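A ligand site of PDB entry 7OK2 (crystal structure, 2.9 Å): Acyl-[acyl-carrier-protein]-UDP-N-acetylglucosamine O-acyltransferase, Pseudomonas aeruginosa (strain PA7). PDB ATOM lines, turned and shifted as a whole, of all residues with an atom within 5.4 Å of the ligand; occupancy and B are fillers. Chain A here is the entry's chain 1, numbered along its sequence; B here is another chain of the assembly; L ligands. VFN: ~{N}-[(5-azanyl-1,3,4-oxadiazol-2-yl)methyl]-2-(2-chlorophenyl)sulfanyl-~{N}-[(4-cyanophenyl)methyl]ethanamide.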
ATOM      1  N   PRO A  72     -16.840  32.149  19.097  1.00  0.00           N
ATOM      2  CA  PRO A  72     -17.168  33.574  19.028  1.00  0.00           C
ATOM      3  C   PRO A  72     -18.151  33.907  20.134  1.00  0.00           C
ATOM      4  O   PRO A  72     -18.357  35.093  20.386  1.00  0.00           O
ATOM      5  CB  PRO A  72     -17.792  33.743  17.647  1.00  0.00           C
ATOM      6  CG  PRO A  72     -17.660  32.401  16.954  1.00  0.00           C
ATOM      7  CD  PRO A  72     -17.554  31.396  18.035  1.00  0.00           C
ATOM      8  N   ASP A  73     -18.693  32.852  20.834  1.00  0.00           N
ATOM      9  CA  ASP A  73     -19.678  32.963  21.927  1.00  0.00           C
ATOM     10  C   ASP A  73     -19.296  33.993  22.940  1.00  0.00           C
ATOM     11  O   ASP A  73     -18.159  34.021  23.410  1.00  0.00           O
ATOM     12  CB  ASP A  73     -19.948  31.627  22.636  1.00  0.00           C
ATOM     13  CG  ASP A  73     -21.421  31.322  22.809  1.00  0.00           C
ATOM     14  OD1 ASP A  73     -21.956  31.584  23.912  1.00  0.00           O
ATOM     15  OD2 ASP A  73     -22.050  30.830  21.849  1.00  0.00           O
ATOM     16  N   LEU A  74     -20.263  34.854  23.255  1.00  0.00           N
ATOM     17  CA  LEU A  74     -20.127  35.954  24.207  1.00  0.00           C
ATOM     18  C   LEU A  74     -19.960  35.412  25.634  1.00  0.00           C
ATOM     19  O   LEU A  74     -19.535  36.135  26.548  1.00  0.00           O
ATOM     20  CB  LEU A  74     -21.331  36.916  24.053  1.00  0.00           C
ATOM     21  CG  LEU A  74     -21.190  38.185  23.150  1.00  0.00           C
ATOM     22  CD1 LEU A  74     -20.451  37.904  21.885  1.00  0.00           C
ATOM     23  CD2 LEU A  74     -22.529  38.759  22.773  1.00  0.00           C
ATOM     24  N   HIS A 121     -19.682  22.218  11.328  1.00  0.00           N
ATOM     25  CA  HIS A 121     -19.311  22.982  12.502  1.00  0.00           C
ATOM     26  C   HIS A 121     -19.405  22.151  13.777  1.00  0.00           C
ATOM     27  O   HIS A 121     -20.508  21.739  14.160  1.00  0.00           O
ATOM     28  CB  HIS A 121     -20.176  24.258  12.584  1.00  0.00           C
ATOM     29  CG  HIS A 121     -19.931  25.074  13.809  1.00  0.00           C
ATOM     30  ND1 HIS A 121     -18.697  25.625  14.062  1.00  0.00           N
ATOM     31  CD2 HIS A 121     -20.768  25.376  14.827  1.00  0.00           C
ATOM     32  CE1 HIS A 121     -18.817  26.258  15.227  1.00  0.00           C
ATOM     33  NE2 HIS A 121     -20.048  26.142  15.714  1.00  0.00           N
ATOM     34  N   HIS A 124     -18.171  24.603  20.402  1.00  0.00           N
ATOM     35  CA  HIS A 124     -17.698  24.496  21.796  1.00  0.00           C
ATOM     36  C   HIS A 124     -18.436  23.493  22.667  1.00  0.00           C
ATOM     37  O   HIS A 124     -19.664  23.426  22.620  1.00  0.00           O
ATOM     38  CB  HIS A 124     -17.728  25.877  22.467  1.00  0.00           C
ATOM     39  CG  HIS A 124     -19.100  26.362  22.852  1.00  0.00           C
ATOM     40  ND1 HIS A 124     -19.964  26.889  21.923  1.00  0.00           N
ATOM     41  CD2 HIS A 124     -19.710  26.361  24.065  1.00  0.00           C
ATOM     42  CE1 HIS A 124     -21.063  27.210  22.587  1.00  0.00           C
ATOM     43  NE2 HIS A 124     -20.953  26.928  23.874  1.00  0.00           N
ATOM     44  N   ALA A 139     -24.120  21.577  11.553  1.00  0.00           N
ATOM     45  CA  ALA A 139     -23.690  22.441  12.638  1.00  0.00           C
ATOM     46  C   ALA A 139     -24.153  22.041  14.004  1.00  0.00           C
ATOM     47  O   ALA A 139     -25.352  21.897  14.203  1.00  0.00           O
ATOM     48  CB  ALA A 139     -24.104  23.868  12.357  1.00  0.00           C
ATOM     49  N   LEU A 140     -23.203  21.877  14.960  1.00  0.00           N
ATOM     50  CA  LEU A 140     -23.499  21.577  16.370  1.00  0.00           C
ATOM     51  C   LEU A 140     -23.311  22.909  17.108  1.00  0.00           C
ATOM     52  O   LEU A 140     -22.213  23.462  17.081  1.00  0.00           O
ATOM     53  CB  LEU A 140     -22.569  20.474  16.943  1.00  0.00           C
ATOM     54  CG  LEU A 140     -22.391  19.156  16.144  1.00  0.00           C
ATOM     55  CD1 LEU A 140     -21.345  18.269  16.772  1.00  0.00           C
ATOM     56  CD2 LEU A 140     -23.664  18.372  16.032  1.00  0.00           C
ATOM     57  N   ALA A 141     -24.388  23.459  17.697  1.00  0.00           N
ATOM     58  CA  ALA A 141     -24.380  24.779  18.369  1.00  0.00           C
ATOM     59  C   ALA A 141     -23.448  24.909  19.564  1.00  0.00           C
ATOM     60  O   ALA A 141     -22.873  25.995  19.788  1.00  0.00           O
ATOM     61  CB  ALA A 141     -25.794  25.165  18.779  1.00  0.00           C
ATOM     62  N   GLY A 142     -23.329  23.836  20.321  1.00  0.00           N
ATOM     63  CA  GLY A 142     -22.510  23.767  21.520  1.00  0.00           C
ATOM     64  C   GLY A 142     -23.061  22.743  22.484  1.00  0.00           C
ATOM     65  O   GLY A 142     -24.260  22.484  22.493  1.00  0.00           O
ATOM     66  N   LEU A 157     -28.673  20.604  11.461  1.00  0.00           N
ATOM     67  CA  LEU A 157     -28.342  21.599  12.461  1.00  0.00           C
ATOM     68  C   LEU A 157     -28.818  21.101  13.815  1.00  0.00           C
ATOM     69  O   LEU A 157     -29.920  20.581  13.959  1.00  0.00           O
ATOM     70  CB  LEU A 157     -28.926  22.983  12.119  1.00  0.00           C
ATOM     71  CG  LEU A 157     -28.873  23.460  10.660  1.00  0.00           C
ATOM     72  CD1 LEU A 157     -29.657  24.733  10.461  1.00  0.00           C
ATOM     73  CD2 LEU A 157     -27.471  23.679  10.227  1.00  0.00           C
ATOM     74  N   VAL A 158     -27.950  21.224  14.802  1.00  0.00           N
ATOM     75  CA  VAL A 158     -28.261  20.775  16.128  1.00  0.00           C
ATOM     76  C   VAL A 158     -28.194  21.926  17.084  1.00  0.00           C
ATOM     77  O   VAL A 158     -27.193  22.632  17.133  1.00  0.00           O
ATOM     78  CB  VAL A 158     -27.371  19.590  16.594  1.00  0.00           C
ATOM     79  CG1 VAL A 158     -28.058  18.830  17.699  1.00  0.00           C
ATOM     80  CG2 VAL A 158     -27.058  18.652  15.435  1.00  0.00           C
ATOM     81  N   HIS A 159     -29.270  22.115  17.833  1.00  0.00           N
ATOM     82  CA  HIS A 159     -29.431  23.127  18.871  1.00  0.00           C
ATOM     83  C   HIS A 159     -28.537  22.728  20.032  1.00  0.00           C
ATOM     84  O   HIS A 159     -28.289  21.543  20.225  1.00  0.00           O
ATOM     85  CB  HIS A 159     -30.889  23.176  19.376  1.00  0.00           C
ATOM     86  CG  HIS A 159     -31.723  24.273  18.774  1.00  0.00           C
ATOM     87  ND1 HIS A 159     -31.195  25.538  18.528  1.00  0.00           N
ATOM     88  CD2 HIS A 159     -33.036  24.281  18.449  1.00  0.00           C
ATOM     89  CE1 HIS A 159     -32.192  26.254  18.029  1.00  0.00           C
ATOM     90  NE2 HIS A 159     -33.322  25.538  17.960  1.00  0.00           N
ATOM     91  N   GLN A 160     -28.113  23.722  20.834  1.00  0.00           N
ATOM     92  CA  GLN A 160     -27.255  23.539  21.994  1.00  0.00           C
ATOM     93  C   GLN A 160     -27.807  22.522  22.980  1.00  0.00           C
ATOM     94  O   GLN A 160     -29.022  22.449  23.177  1.00  0.00           O
ATOM     95  CB  GLN A 160     -27.044  24.886  22.706  1.00  0.00           C
ATOM     96  CG  GLN A 160     -25.606  25.194  23.110  1.00  0.00           C
ATOM     97  CD  GLN A 160     -25.319  26.639  23.457  1.00  0.00           C
ATOM     98  OE1 GLN A 160     -24.250  26.992  23.985  1.00  0.00           O
ATOM     99  NE2 GLN A 160     -26.246  27.524  23.149  1.00  0.00           N
ATOM    100  N   LEU B 115     -21.301  41.040  15.634  1.00  0.00           N
ATOM    101  CA  LEU B 115     -20.699  39.731  15.686  1.00  0.00           C
ATOM    102  C   LEU B 115     -21.216  38.983  14.470  1.00  0.00           C
ATOM    103  O   LEU B 115     -22.361  38.548  14.438  1.00  0.00           O
ATOM    104  CB  LEU B 115     -20.982  38.981  17.009  1.00  0.00           C
ATOM    105  CG  LEU B 115     -20.398  37.561  17.146  1.00  0.00           C
ATOM    106  CD1 LEU B 115     -18.889  37.524  16.977  1.00  0.00           C
ATOM    107  CD2 LEU B 115     -20.756  36.964  18.467  1.00  0.00           C
ATOM    108  N   MET B 117     -20.687  35.754  12.597  1.00  0.00           N
ATOM    109  CA  MET B 117     -20.130  34.414  12.836  1.00  0.00           C
ATOM    110  C   MET B 117     -19.686  33.714  11.550  1.00  0.00           C
ATOM    111  O   MET B 117     -20.078  34.133  10.448  1.00  0.00           O
ATOM    112  CB  MET B 117     -21.147  33.551  13.606  1.00  0.00           C
ATOM    113  CG  MET B 117     -20.624  32.966  14.881  1.00  0.00           C
ATOM    114  SD  MET B 117     -21.697  33.329  16.289  1.00  0.00           S
ATOM    115  CE  MET B 117     -21.400  31.834  17.306  1.00  0.00           C
ATOM    116  N   ILE B 133     -25.928  39.965  16.337  1.00  0.00           N
ATOM    117  CA  ILE B 133     -25.221  38.688  16.267  1.00  0.00           C
ATOM    118  C   ILE B 133     -25.786  37.968  15.007  1.00  0.00           C
ATOM    119  O   ILE B 133     -27.010  37.929  14.804  1.00  0.00           O
ATOM    120  CB  ILE B 133     -25.463  37.855  17.550  1.00  0.00           C
ATOM    121  CG1 ILE B 133     -24.780  38.504  18.769  1.00  0.00           C
ATOM    122  CG2 ILE B 133     -25.019  36.409  17.350  1.00  0.00           C
ATOM    123  CD1 ILE B 133     -25.449  38.226  20.109  1.00  0.00           C
ATOM    124  N   VAL B 135     -25.253  34.456  13.497  1.00  0.00           N
ATOM    125  CA  VAL B 135     -24.746  33.117  13.746  1.00  0.00           C
ATOM    126  C   VAL B 135     -24.331  32.425  12.414  1.00  0.00           C
ATOM    127  O   VAL B 135     -24.558  32.964  11.318  1.00  0.00           O
ATOM    128  CB  VAL B 135     -25.736  32.306  14.624  1.00  0.00           C
ATOM    129  CG1 VAL B 135     -25.152  30.990  15.059  1.00  0.00           C
ATOM    130  CG2 VAL B 135     -26.115  33.109  15.863  1.00  0.00           C
ATOM    131  N   ASN B 136     -23.576  31.316  12.534  1.00  0.00           N
ATOM    132  CA  ASN B 136     -23.006  30.568  11.433  1.00  0.00           C
ATOM    133  C   ASN B 136     -23.885  30.496  10.222  1.00  0.00           C
ATOM    134  O   ASN B 136     -25.077  30.214  10.335  1.00  0.00           O
ATOM    135  CB  ASN B 136     -22.616  29.168  11.886  1.00  0.00           C
ATOM    136  CG  ASN B 136     -21.456  29.120  12.829  1.00  0.00           C
ATOM    137  OD1 ASN B 136     -21.378  29.875  13.817  1.00  0.00           O
ATOM    138  ND2 ASN B 136     -20.532  28.196  12.552  1.00  0.00           N
ATOM    139  N   ILE B 151     -30.852  39.300  16.677  1.00  0.00           N
ATOM    140  CA  ILE B 151     -30.063  38.071  16.772  1.00  0.00           C
ATOM    141  C   ILE B 151     -30.539  37.167  15.662  1.00  0.00           C
ATOM    142  O   ILE B 151     -31.714  36.769  15.655  1.00  0.00           O
ATOM    143  CB  ILE B 151     -30.041  37.388  18.191  1.00  0.00           C
ATOM    144  CG1 ILE B 151     -29.335  38.259  19.233  1.00  0.00           C
ATOM    145  CG2 ILE B 151     -29.369  36.027  18.160  1.00  0.00           C
ATOM    146  CD1 ILE B 151     -30.284  39.030  20.119  1.00  0.00           C
ATOM    147  N   SER B 153     -30.082  33.621  14.184  1.00  0.00           N
ATOM    148  CA  SER B 153     -29.613  32.242  14.483  1.00  0.00           C
ATOM    149  C   SER B 153     -28.941  31.518  13.309  1.00  0.00           C
ATOM    150  O   SER B 153     -29.000  31.976  12.164  1.00  0.00           O
ATOM    151  CB  SER B 153     -30.749  31.397  15.063  1.00  0.00           C
ATOM    152  OG  SER B 153     -31.148  31.722  16.382  1.00  0.00           O
ATOM    153  N   GLY B 154     -28.299  30.384  13.609  1.00  0.00           N
ATOM    154  CA  GLY B 154     -27.586  29.581  12.631  1.00  0.00           C
ATOM    155  C   GLY B 154     -28.359  29.284  11.383  1.00  0.00           C
ATOM    156  O   GLY B 154     -29.523  28.890  11.427  1.00  0.00           O
ATOM    157  N   TYR B 155     -27.705  29.517  10.254  1.00  0.00           N
ATOM    158  CA  TYR B 155     -28.194  29.230   8.903  1.00  0.00           C
ATOM    159  C   TYR B 155     -29.542  29.905   8.590  1.00  0.00           C
ATOM    160  O   TYR B 155     -30.385  29.292   7.927  1.00  0.00           O
ATOM    161  CB  TYR B 155     -28.216  27.695   8.614  1.00  0.00           C
ATOM    162  CG  TYR B 155     -26.862  27.002   8.602  1.00  0.00           C
ATOM    163  CD1 TYR B 155     -26.075  26.938   9.746  1.00  0.00           C
ATOM    164  CD2 TYR B 155     -26.418  26.324   7.468  1.00  0.00           C
ATOM    165  CE1 TYR B 155     -24.844  26.276   9.744  1.00  0.00           C
ATOM    166  CE2 TYR B 155     -25.191  25.650   7.459  1.00  0.00           C
ATOM    167  CZ  TYR B 155     -24.401  25.627   8.602  1.00  0.00           C
ATOM    168  OH  TYR B 155     -23.168  25.025   8.593  1.00  0.00           O
ATOM    169  N   PHE B 169     -35.503  38.430  16.587  1.00  0.00           N
ATOM    170  CA  PHE B 169     -34.763  37.172  16.621  1.00  0.00           C
ATOM    171  C   PHE B 169     -35.313  36.128  15.651  1.00  0.00           C
ATOM    172  O   PHE B 169     -36.517  35.857  15.654  1.00  0.00           O
ATOM    173  CB  PHE B 169     -34.794  36.620  18.069  1.00  0.00           C
ATOM    174  CG  PHE B 169     -34.226  35.253  18.289  1.00  0.00           C
ATOM    175  CD1 PHE B 169     -34.972  34.111  18.030  1.00  0.00           C
ATOM    176  CD2 PHE B 169     -32.946  35.087  18.832  1.00  0.00           C
ATOM    177  CE1 PHE B 169     -34.429  32.840  18.221  1.00  0.00           C
ATOM    178  CE2 PHE B 169     -32.414  33.822  19.048  1.00  0.00           C
ATOM    179  CZ  PHE B 169     -33.158  32.698  18.739  1.00  0.00           C
ATOM    180  N   MET B 172     -32.960  28.974  14.379  1.00  0.00           N
ATOM    181  CA  MET B 172     -32.045  28.383  13.399  1.00  0.00           C
ATOM    182  C   MET B 172     -32.771  27.802  12.168  1.00  0.00           C
ATOM    183  O   MET B 172     -33.885  27.303  12.277  1.00  0.00           O
ATOM    184  CB  MET B 172     -31.037  27.377  14.011  1.00  0.00           C
ATOM    185  CG  MET B 172     -31.593  26.065  14.464  1.00  0.00           C
ATOM    186  SD  MET B 172     -30.219  25.039  14.968  1.00  0.00           S
ATOM    187  CE  MET B 172     -31.044  23.581  15.219  1.00  0.00           C
HETATM  188  C15 VFN L   1     -23.901  34.428  20.747  1.00  0.00           C
HETATM  189  C23 VFN L   1     -23.871  28.503  17.077  1.00  0.00           C
HETATM  190  C24 VFN L   1     -23.235  28.081  15.910  1.00  0.00           C
HETATM  191  C11 VFN L   1     -26.315  34.151  20.812  1.00  0.00           C
HETATM  192  C13 VFN L   1     -24.960  32.689  19.421  1.00  0.00           C
HETATM  193  C10 VFN L   1     -27.499  33.506  20.407  1.00  0.00           C
HETATM  194  C14 VFN L   1     -26.141  32.048  19.025  1.00  0.00           C
HETATM  195  C22 VFN L   1     -25.254  28.297  17.183  1.00  0.00           C
HETATM  196  C25 VFN L   1     -23.973  27.476  14.894  1.00  0.00           C
HETATM  197  C12 VFN L   1     -25.065  33.747  20.321  1.00  0.00           C
HETATM  198  C9  VFN L   1     -27.398  32.446  19.499  1.00  0.00           C
HETATM  199  C21 VFN L   1     -26.028  27.686  16.185  1.00  0.00           C
HETATM  200  C26 VFN L   1     -25.348  27.275  15.017  1.00  0.00           C
HETATM  201  C5  VFN L   1     -27.211  29.769  21.053  1.00  0.00           C
HETATM  202  C2  VFN L   1     -25.124  29.406  21.147  1.00  0.00           C
HETATM  203  C17 VFN L   1     -28.401  29.635  17.897  1.00  0.00           C
HETATM  204  C8  VFN L   1     -28.647  31.754  19.079  1.00  0.00           C
HETATM  205  C6  VFN L   1     -28.542  29.675  20.439  1.00  0.00           C
HETATM  206  C19 VFN L   1     -28.258  28.139  17.955  1.00  0.00           C
HETATM  207  N16 VFN L   1     -22.946  34.985  21.085  1.00  0.00           N
HETATM  208  N4  VFN L   1     -26.783  30.454  22.090  1.00  0.00           N
HETATM  209  N3  VFN L   1     -25.431  30.201  22.165  1.00  0.00           N
HETATM  210  N1  VFN L   1     -23.944  28.855  20.728  1.00  0.00           N
HETATM  211  N7  VFN L   1     -28.514  30.307  19.127  1.00  0.00           N
HETATM  212  O18 VFN L   1     -28.399  30.209  16.827  1.00  0.00           O
HETATM  213  O28 VFN L   1     -26.222  29.086  20.407  1.00  0.00           O
HETATM  214  S20 VFN L   1     -27.794  27.452  16.341  1.00  0.00           S
HETATM  215 CL1  VFN L   1     -26.173  26.505  13.715  1.00  0.00          CL
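OD2 of Asp 73 sits at hydrogen-bond distance from N1 of the ligand (3.0 Å).
The side-chain amide nitrogen of Gln 160 sits at hydrogen-bond distance from a nitrogen (N3) of the ligand, 3.0 Å away.
An oxygen (O18) of the ligand lies within hydrogen-bond range of the backbone NH (N) of Gly 154 of chain B, at 3.2 Å.
N of Leu 74 is in hydrogen-bond range of N16 of the ligand.
The backbone carbonyl oxygen (O) of Ala 141 sits at hydrogen-bond distance from a nitrogen (N1) of the ligand (3.2 Å).
The side-chain hydroxyl (OG) of Ser 153 of chain B sits at hydrogen-bond distance from an oxygen (O18) of the ligand (3.2 Å).
The backbone NH (N) of Leu 140 is in hydrogen-bond range of the backbone carbonyl oxygen (O) of His 121 (2.8 Å).
The backbone NH (N) of Ala 141 lies within hydrogen-bond range of the backbone carbonyl oxygen (O) of Val 158 (3.0 Å).
A ring nitrogen (NE2) of His 124 sits at hydrogen-bond distance from the side-chain amide oxygen of Gln 160 (3.3 Å).
N of Val 158 sits at hydrogen-bond distance from O of Ala 139 (2.7 Å).
O of Asn 136 of chain B is in hydrogen-bond range of N of Tyr 155 of chain B.
SD of Met 172 of chain B lies within hydrogen-bond range of ND1 of His 159 (3.7 Å).
A sulfur (S20) of the ligand lies close to the side-chain sulfur (SD) of Met 172 of chain B (3.7 Å).
Residues that only touch the ligand: Asn 136 of chain B (3.3 Å), Val 135 of chain B (3.3 Å), Ala 139 (3.6 Å), His 121 (3.7 Å), His 124 (3.8 Å), Ile 151 of chain B (3.9 Å), Leu 115 of chain B (3.9 Å), His 159 (3.96 Å), Ile 133 of chain B (3.99 Å) and Tyr 155 of chain B (3.99 Å).
Of the 24 residues printed, 17 come within 4 Å of the ligand.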
